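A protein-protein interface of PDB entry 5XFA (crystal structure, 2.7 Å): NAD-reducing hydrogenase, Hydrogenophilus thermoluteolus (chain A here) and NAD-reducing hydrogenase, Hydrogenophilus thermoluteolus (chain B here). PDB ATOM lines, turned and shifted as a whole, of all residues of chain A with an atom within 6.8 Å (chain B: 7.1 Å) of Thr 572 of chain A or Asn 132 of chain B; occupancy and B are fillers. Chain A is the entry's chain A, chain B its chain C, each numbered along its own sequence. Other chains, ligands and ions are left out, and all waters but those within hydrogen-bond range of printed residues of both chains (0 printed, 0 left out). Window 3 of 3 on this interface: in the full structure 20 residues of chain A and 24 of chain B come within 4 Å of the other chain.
The backbone carbonyl oxygen (O) of Thr 572 of chain A lies within hydrogen-bond range of the side-chain amide nitrogen (ND2) of Asn 132 of chain B.
O of Asp 133 of chain B lies within hydrogen-bond range of NH1 of Arg 574 of chain A, 3.4 Å away.
The guanidinium group of Arg 574 of chain A sits close to the backbone carbonyl oxygen of Pro 134 of chain B (3.3 Å).
The guanidinium group (NH1) of Arg 574 of chain A sits at hydrogen-bond distance from the backbone carbonyl oxygen (O) of Leu 136 of chain B.
NH1 of Arg 569 of chain A is in hydrogen-bond range of O of Ala 579 of chain A (2.6 Å).
OG1 of Thr 572 of chain A sits close to N of Arg 574 of chain A.
OD1 of Asp 576 of chain A is in salt-bridge range of NE of Arg 574 of chain A, 3.0 Å away.
The side-chain carboxylate (OE2) of Glu 119 of chain B is in hydrogen-bond range of the backbone NH (N) of Val 130 of chain B, 3.3 Å away.
The side-chain amide oxygen (OD1) of Asn 132 of chain B lies close to the backbone carbonyl oxygen (O) of Val 130 of chain B (2.8 Å).
The side-chain carboxylate of Asp 133 of chain B sits at hydrogen-bond distance from the backbone NH of Glu 135 of chain B.
Among the printed residues, pairs that only touch across the chains: Thr 568 of chain A with Leu 114 of chain B (3.9 Å), Thr 568 of chain A with Leu 138 of chain B (3.5 Å), Arg 569 of chain A with Leu 138 of chain B (3.3 Å), Leu 571 of chain A with Leu 114 of chain B (3.99 Å), Leu 571 of chain A with Val 130 of chain B (3.9 Å), Thr 572 of chain A with Pro 131 of chain B (3.6 Å), Arg 574 of chain A with Asn 132 of chain B (3.1 Å) and Arg 574 of chain A with Leu 138 of chain B (2.9 Å).
Printed residues of chain B within 4 Å of Thr 572 of chain A: Pro 131 (3.6 Å) and Asn 132 (3.2 Å).
Of chain A, only Thr 572 (3.2 Å) and Arg 574 (3.1 Å) come within 4 Å of Asn 132 of chain B.
Of the printed residues of chain A, Pro 131 of chain B touches Thr 572 (3.6 Å).
Of the printed residues of chain A, Val 130 of chain B touches Leu 571.
Printed residues of chain A within 4 Å of Pro 134 of chain B: Arg 574.
Of the printed residues of chain A, Leu 136 of chain B touches Arg 574 (2.7 Å).
Printed residues of chain B within 4 Å of Thr 568 of chain A: Leu 114 (3.9 Å) and Leu 138 (3.5 Å).
The nearest residue of chain A that does not touch Asn 132 of chain B is Leu 571 of chain A (5.1 Å).
The nearest printed residue of chain A that does not touch Leu 138 of chain B is Ala 579 of chain A (4.004 Å).
Hydrophobic or aromatic side chains of chain B that line the printed part of chain A: Leu 114, Val 130, Pro 134 and Leu 138.
Of the 11 printed residues of chain A, 5 touch a printed residue of chain B.
Printed residues of chain A that touch a printed residue of chain B: Thr 568, Arg 569, Leu 571, Thr 572 and Arg 574.
Hydrophobic or aromatic side chains of chain A that line the printed part of chain B: Leu 571.
Among the printed residues, no Asp or Glu carboxylate lies within 4 Å of a Lys or Arg side-chain nitrogen of the other chain.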
ATOM      1  N   ALA A 567       7.824 -12.013 -38.462  1.00  0.00           N
ATOM      2  CA  ALA A 567       6.823 -12.958 -37.979  1.00  0.00           C
ATOM      3  C   ALA A 567       6.976 -13.301 -36.480  1.00  0.00           C
ATOM      4  O   ALA A 567       5.995 -13.321 -35.726  1.00  0.00           O
ATOM      5  CB  ALA A 567       6.889 -14.236 -38.813  1.00  0.00           C
ATOM      6  N   THR A 568       8.209 -13.598 -36.072  1.00  0.00           N
ATOM      7  CA  THR A 568       8.505 -13.999 -34.699  1.00  0.00           C
ATOM      8  C   THR A 568       8.619 -12.804 -33.766  1.00  0.00           C
ATOM      9  O   THR A 568       8.299 -12.924 -32.584  1.00  0.00           O
ATOM     10  CB  THR A 568       9.778 -14.856 -34.627  1.00  0.00           C
ATOM     11  OG1 THR A 568      10.678 -14.473 -35.672  1.00  0.00           O
ATOM     12  CG2 THR A 568       9.430 -16.307 -34.810  1.00  0.00           C
ATOM     13  N   ARG A 569       9.042 -11.649 -34.280  1.00  0.00           N
ATOM     14  CA  ARG A 569       8.873 -10.398 -33.508  1.00  0.00           C
ATOM     15  C   ARG A 569       7.393 -10.135 -33.146  1.00  0.00           C
ATOM     16  O   ARG A 569       7.063  -9.982 -31.980  1.00  0.00           O
ATOM     17  CB  ARG A 569       9.482  -9.193 -34.229  1.00  0.00           C
ATOM     18  CG  ARG A 569      10.967  -8.999 -33.929  1.00  0.00           C
ATOM     19  CD  ARG A 569      11.434  -7.620 -34.331  1.00  0.00           C
ATOM     20  NE  ARG A 569      11.170  -7.379 -35.749  1.00  0.00           N
ATOM     21  CZ  ARG A 569      12.028  -7.608 -36.735  1.00  0.00           C
ATOM     22  NH1 ARG A 569      13.251  -8.080 -36.479  1.00  0.00           N
ATOM     23  NH2 ARG A 569      11.663  -7.354 -37.987  1.00  0.00           N
ATOM     24  N   ARG A 570       6.506 -10.110 -34.143  1.00  0.00           N
ATOM     25  CA  ARG A 570       5.078  -9.962 -33.889  1.00  0.00           C
ATOM     26  C   ARG A 570       4.630 -10.871 -32.737  1.00  0.00           C
ATOM     27  O   ARG A 570       3.978 -10.412 -31.808  1.00  0.00           O
ATOM     28  CB  ARG A 570       4.273 -10.242 -35.167  1.00  0.00           C
ATOM     29  CG  ARG A 570       2.755 -10.119 -35.006  1.00  0.00           C
ATOM     30  CD  ARG A 570       2.083  -9.363 -36.155  1.00  0.00           C
ATOM     31  NE  ARG A 570       0.963  -8.517 -35.702  1.00  0.00           N
ATOM     32  CZ  ARG A 570       1.058  -7.254 -35.251  1.00  0.00           C
ATOM     33  NH1 ARG A 570       2.230  -6.620 -35.160  1.00  0.00           N
ATOM     34  NH2 ARG A 570      -0.046  -6.609 -34.877  1.00  0.00           N
ATOM     35  N   LEU A 571       5.013 -12.145 -32.782  1.00  0.00           N
ATOM     36  CA  LEU A 571       4.503 -13.151 -31.847  1.00  0.00           C
ATOM     37  C   LEU A 571       5.050 -12.987 -30.429  1.00  0.00           C
ATOM     38  O   LEU A 571       4.285 -12.873 -29.482  1.00  0.00           O
ATOM     39  CB  LEU A 571       4.853 -14.536 -32.365  1.00  0.00           C
ATOM     40  CG  LEU A 571       4.151 -15.744 -31.723  1.00  0.00           C
ATOM     41  CD1 LEU A 571       2.698 -15.802 -32.168  1.00  0.00           C
ATOM     42  CD2 LEU A 571       4.850 -17.060 -32.067  1.00  0.00           C
ATOM     43  N   THR A 572       6.374 -12.971 -30.286  1.00  0.00           N
ATOM     44  CA  THR A 572       7.017 -12.840 -28.973  1.00  0.00           C
ATOM     45  C   THR A 572       6.817 -11.456 -28.363  1.00  0.00           C
ATOM     46  O   THR A 572       6.839 -11.300 -27.148  1.00  0.00           O
ATOM     47  CB  THR A 572       8.541 -13.070 -29.061  1.00  0.00           C
ATOM     48  OG1 THR A 572       9.119 -12.124 -29.964  1.00  0.00           O
ATOM     49  CG2 THR A 572       8.849 -14.486 -29.534  1.00  0.00           C
ATOM     50  N   GLY A 573       6.663 -10.459 -29.227  1.00  0.00           N
ATOM     51  CA  GLY A 573       6.461  -9.081 -28.823  1.00  0.00           C
ATOM     52  C   GLY A 573       7.752  -8.329 -28.564  1.00  0.00           C
ATOM     53  O   GLY A 573       7.745  -7.370 -27.800  1.00  0.00           O
ATOM     54  N   ARG A 574       8.850  -8.719 -29.203  1.00  0.00           N
ATOM     55  CA  ARG A 574      10.129  -8.031 -28.945  1.00  0.00           C
ATOM     56  C   ARG A 574      10.544  -7.056 -30.041  1.00  0.00           C
ATOM     57  O   ARG A 574      10.185  -7.205 -31.219  1.00  0.00           O
ATOM     58  CB  ARG A 574      11.296  -8.979 -28.618  1.00  0.00           C
ATOM     59  CG  ARG A 574      10.996 -10.460 -28.717  1.00  0.00           C
ATOM     60  CD  ARG A 574      11.899 -11.275 -27.801  1.00  0.00           C
ATOM     61  NE  ARG A 574      13.321 -11.034 -28.042  1.00  0.00           N
ATOM     62  CZ  ARG A 574      14.234 -11.982 -28.256  1.00  0.00           C
ATOM     63  NH1 ARG A 574      13.908 -13.275 -28.252  1.00  0.00           N
ATOM     64  NH2 ARG A 574      15.504 -11.643 -28.433  1.00  0.00           N
ATOM     65  N   ASP A 575      11.281  -6.040 -29.608  1.00  0.00           N
ATOM     66  CA  ASP A 575      11.946  -5.122 -30.515  1.00  0.00           C
ATOM     67  C   ASP A 575      13.350  -4.751 -30.019  1.00  0.00           C
ATOM     68  O   ASP A 575      13.937  -3.779 -30.500  1.00  0.00           O
ATOM     69  CB  ASP A 575      11.096  -3.860 -30.717  1.00  0.00           C
ATOM     70  CG  ASP A 575      11.408  -3.141 -32.040  1.00  0.00           C
ATOM     71  OD1 ASP A 575      11.179  -3.735 -33.123  1.00  0.00           O
ATOM     72  OD2 ASP A 575      11.866  -1.975 -31.998  1.00  0.00           O
ATOM     73  N   ASP A 576      13.889  -5.519 -29.071  1.00  0.00           N
ATOM     74  CA  ASP A 576      15.275  -5.348 -28.634  1.00  0.00           C
ATOM     75  C   ASP A 576      16.268  -5.624 -29.792  1.00  0.00           C
ATOM     76  O   ASP A 576      15.908  -6.275 -30.770  1.00  0.00           O
ATOM     77  CB  ASP A 576      15.572  -6.274 -27.451  1.00  0.00           C
ATOM     78  CG  ASP A 576      15.248  -7.742 -27.746  1.00  0.00           C
ATOM     79  OD1 ASP A 576      14.035  -8.110 -27.719  1.00  0.00           O
ATOM     80  OD2 ASP A 576      16.215  -8.519 -27.975  1.00  0.00           O
ATOM     81  N   ALA A 579      16.640  -9.133 -31.368  1.00  0.00           N
ATOM     82  CA  ALA A 579      15.538  -9.601 -32.239  1.00  0.00           C
ATOM     83  C   ALA A 579      15.557  -8.948 -33.630  1.00  0.00           C
ATOM     84  O   ALA A 579      14.517  -8.889 -34.317  1.00  0.00           O
ATOM     85  CB  ALA A 579      14.194  -9.339 -31.580  1.00  0.00           C
ATOM     86  N   LEU B 114       5.034 -22.633 -33.811  1.00  0.00           N
ATOM     87  CA  LEU B 114       5.403 -22.381 -32.421  1.00  0.00           C
ATOM     88  C   LEU B 114       4.177 -22.437 -31.536  1.00  0.00           C
ATOM     89  O   LEU B 114       4.216 -22.898 -30.385  1.00  0.00           O
ATOM     90  CB  LEU B 114       6.064 -21.013 -32.301  1.00  0.00           C
ATOM     91  CG  LEU B 114       7.494 -20.915 -32.834  1.00  0.00           C
ATOM     92  CD1 LEU B 114       7.855 -19.467 -33.126  1.00  0.00           C
ATOM     93  CD2 LEU B 114       8.485 -21.501 -31.850  1.00  0.00           C
ATOM     94  N   GLU B 119       1.575 -23.703 -27.347  1.00  0.00           N
ATOM     95  CA  GLU B 119       0.298 -23.205 -26.842  1.00  0.00           C
ATOM     96  C   GLU B 119      -0.860 -24.160 -27.046  1.00  0.00           C
ATOM     97  O   GLU B 119      -1.662 -24.370 -26.129  1.00  0.00           O
ATOM     98  CB  GLU B 119      -0.049 -21.852 -27.469  1.00  0.00           C
ATOM     99  CG  GLU B 119       0.910 -20.726 -27.075  1.00  0.00           C
ATOM    100  CD  GLU B 119       0.425 -19.327 -27.455  1.00  0.00           C
ATOM    101  OE1 GLU B 119      -0.748 -19.200 -27.888  1.00  0.00           O
ATOM    102  OE2 GLU B 119       1.228 -18.361 -27.339  1.00  0.00           O
ATOM    103  N   ARG B 129       2.523 -20.617 -22.977  1.00  0.00           N
ATOM    104  CA  ARG B 129       2.702 -19.638 -24.058  1.00  0.00           C
ATOM    105  C   ARG B 129       4.054 -19.805 -24.744  1.00  0.00           C
ATOM    106  O   ARG B 129       5.021 -20.261 -24.120  1.00  0.00           O
ATOM    107  CB  ARG B 129       2.539 -18.206 -23.533  1.00  0.00           C
ATOM    108  CG  ARG B 129       1.140 -17.911 -22.995  1.00  0.00           C
ATOM    109  CD  ARG B 129       0.730 -16.450 -23.152  1.00  0.00           C
ATOM    110  NE  ARG B 129       0.264 -16.154 -24.517  1.00  0.00           N
ATOM    111  CZ  ARG B 129       0.831 -15.298 -25.377  1.00  0.00           C
ATOM    112  NH1 ARG B 129       1.916 -14.596 -25.045  1.00  0.00           N
ATOM    113  NH2 ARG B 129       0.302 -15.136 -26.592  1.00  0.00           N
ATOM    114  N   VAL B 130       4.103 -19.444 -26.023  1.00  0.00           N
ATOM    115  CA  VAL B 130       5.342 -19.436 -26.801  1.00  0.00           C
ATOM    116  C   VAL B 130       6.406 -18.652 -26.030  1.00  0.00           C
ATOM    117  O   VAL B 130       6.127 -17.570 -25.519  1.00  0.00           O
ATOM    118  CB  VAL B 130       5.157 -18.735 -28.171  1.00  0.00           C
ATOM    119  CG1 VAL B 130       6.498 -18.566 -28.879  1.00  0.00           C
ATOM    120  CG2 VAL B 130       4.170 -19.487 -29.064  1.00  0.00           C
ATOM    121  N   PRO B 131       7.625 -19.192 -25.938  1.00  0.00           N
ATOM    122  CA  PRO B 131       8.694 -18.488 -25.223  1.00  0.00           C
ATOM    123  C   PRO B 131       9.047 -17.127 -25.789  1.00  0.00           C
ATOM    124  O   PRO B 131       9.251 -17.023 -26.987  1.00  0.00           O
ATOM    125  CB  PRO B 131       9.872 -19.449 -25.355  1.00  0.00           C
ATOM    126  CG  PRO B 131       9.233 -20.802 -25.361  1.00  0.00           C
ATOM    127  CD  PRO B 131       7.947 -20.620 -26.127  1.00  0.00           C
ATOM    128  N   ASN B 132       9.132 -16.125 -24.908  1.00  0.00           N
ATOM    129  CA  ASN B 132       9.258 -14.690 -25.219  1.00  0.00           C
ATOM    130  C   ASN B 132      10.619 -14.108 -24.925  1.00  0.00           C
ATOM    131  O   ASN B 132      10.926 -13.006 -25.365  1.00  0.00           O
ATOM    132  CB  ASN B 132       8.360 -13.889 -24.282  1.00  0.00           C
ATOM    133  CG  ASN B 132       6.918 -13.872 -24.703  1.00  0.00           C
ATOM    134  OD1 ASN B 132       6.401 -14.833 -25.260  1.00  0.00           O
ATOM    135  ND2 ASN B 132       6.245 -12.770 -24.423  1.00  0.00           N
ATOM    136  N   ASP B 133      11.399 -14.788 -24.093  1.00  0.00           N
ATOM    137  CA  ASP B 133      12.526 -14.150 -23.453  1.00  0.00           C
ATOM    138  C   ASP B 133      13.655 -13.851 -24.453  1.00  0.00           C
ATOM    139  O   ASP B 133      14.106 -14.745 -25.165  1.00  0.00           O
ATOM    140  CB  ASP B 133      13.034 -15.018 -22.314  1.00  0.00           C
ATOM    141  CG  ASP B 133      14.110 -14.331 -21.484  1.00  0.00           C
ATOM    142  OD1 ASP B 133      15.130 -13.902 -22.064  1.00  0.00           O
ATOM    143  OD2 ASP B 133      13.952 -14.249 -20.243  1.00  0.00           O
ATOM    144  N   PRO B 134      14.117 -12.588 -24.498  1.00  0.00           N
ATOM    145  CA  PRO B 134      15.268 -12.156 -25.272  1.00  0.00           C
ATOM    146  C   PRO B 134      16.510 -13.049 -25.227  1.00  0.00           C
ATOM    147  O   PRO B 134      17.379 -12.904 -26.076  1.00  0.00           O
ATOM    148  CB  PRO B 134      15.596 -10.792 -24.667  1.00  0.00           C
ATOM    149  CG  PRO B 134      14.278 -10.258 -24.274  1.00  0.00           C
ATOM    150  CD  PRO B 134      13.485 -11.450 -23.804  1.00  0.00           C
ATOM    151  N   GLU B 135      16.625 -13.933 -24.245  1.00  0.00           N
ATOM    152  CA  GLU B 135      17.740 -14.886 -24.215  1.00  0.00           C
ATOM    153  C   GLU B 135      17.573 -15.922 -25.340  1.00  0.00           C
ATOM    154  O   GLU B 135      18.542 -16.448 -25.885  1.00  0.00           O
ATOM    155  CB  GLU B 135      17.843 -15.568 -22.841  1.00  0.00           C
ATOM    156  CG  GLU B 135      18.032 -14.621 -21.656  1.00  0.00           C
ATOM    157  CD  GLU B 135      19.474 -14.207 -21.407  1.00  0.00           C
ATOM    158  OE1 GLU B 135      20.315 -14.309 -22.330  1.00  0.00           O
ATOM    159  OE2 GLU B 135      19.764 -13.751 -20.272  1.00  0.00           O
ATOM    160  N   LEU B 136      16.332 -16.206 -25.694  1.00  0.00           N
ATOM    161  CA  LEU B 136      16.071 -17.091 -26.817  1.00  0.00           C
ATOM    162  C   LEU B 136      16.179 -16.329 -28.149  1.00  0.00           C
ATOM    163  O   LEU B 136      15.790 -15.161 -28.228  1.00  0.00           O
ATOM    164  CB  LEU B 136      14.708 -17.751 -26.650  1.00  0.00           C
ATOM    165  CG  LEU B 136      14.556 -18.481 -25.310  1.00  0.00           C
ATOM    166  CD1 LEU B 136      13.256 -19.242 -25.302  1.00  0.00           C
ATOM    167  CD2 LEU B 136      15.715 -19.423 -25.053  1.00  0.00           C
ATOM    168  N   LEU B 138      15.137 -15.629 -32.046  1.00  0.00           N
ATOM    169  CA  LEU B 138      13.935 -15.747 -32.860  1.00  0.00           C
ATOM    170  C   LEU B 138      14.204 -16.610 -34.080  1.00  0.00           C
ATOM    171  O   LEU B 138      15.232 -16.474 -34.743  1.00  0.00           O
ATOM    172  CB  LEU B 138      13.438 -14.362 -33.310  1.00  0.00           C
ATOM    173  CG  LEU B 138      12.524 -13.635 -32.329  1.00  0.00           C
ATOM    174  CD1 LEU B 138      13.267 -13.305 -31.054  1.00  0.00           C
ATOM    175  CD2 LEU B 138      11.951 -12.363 -32.943  1.00  0.00           C
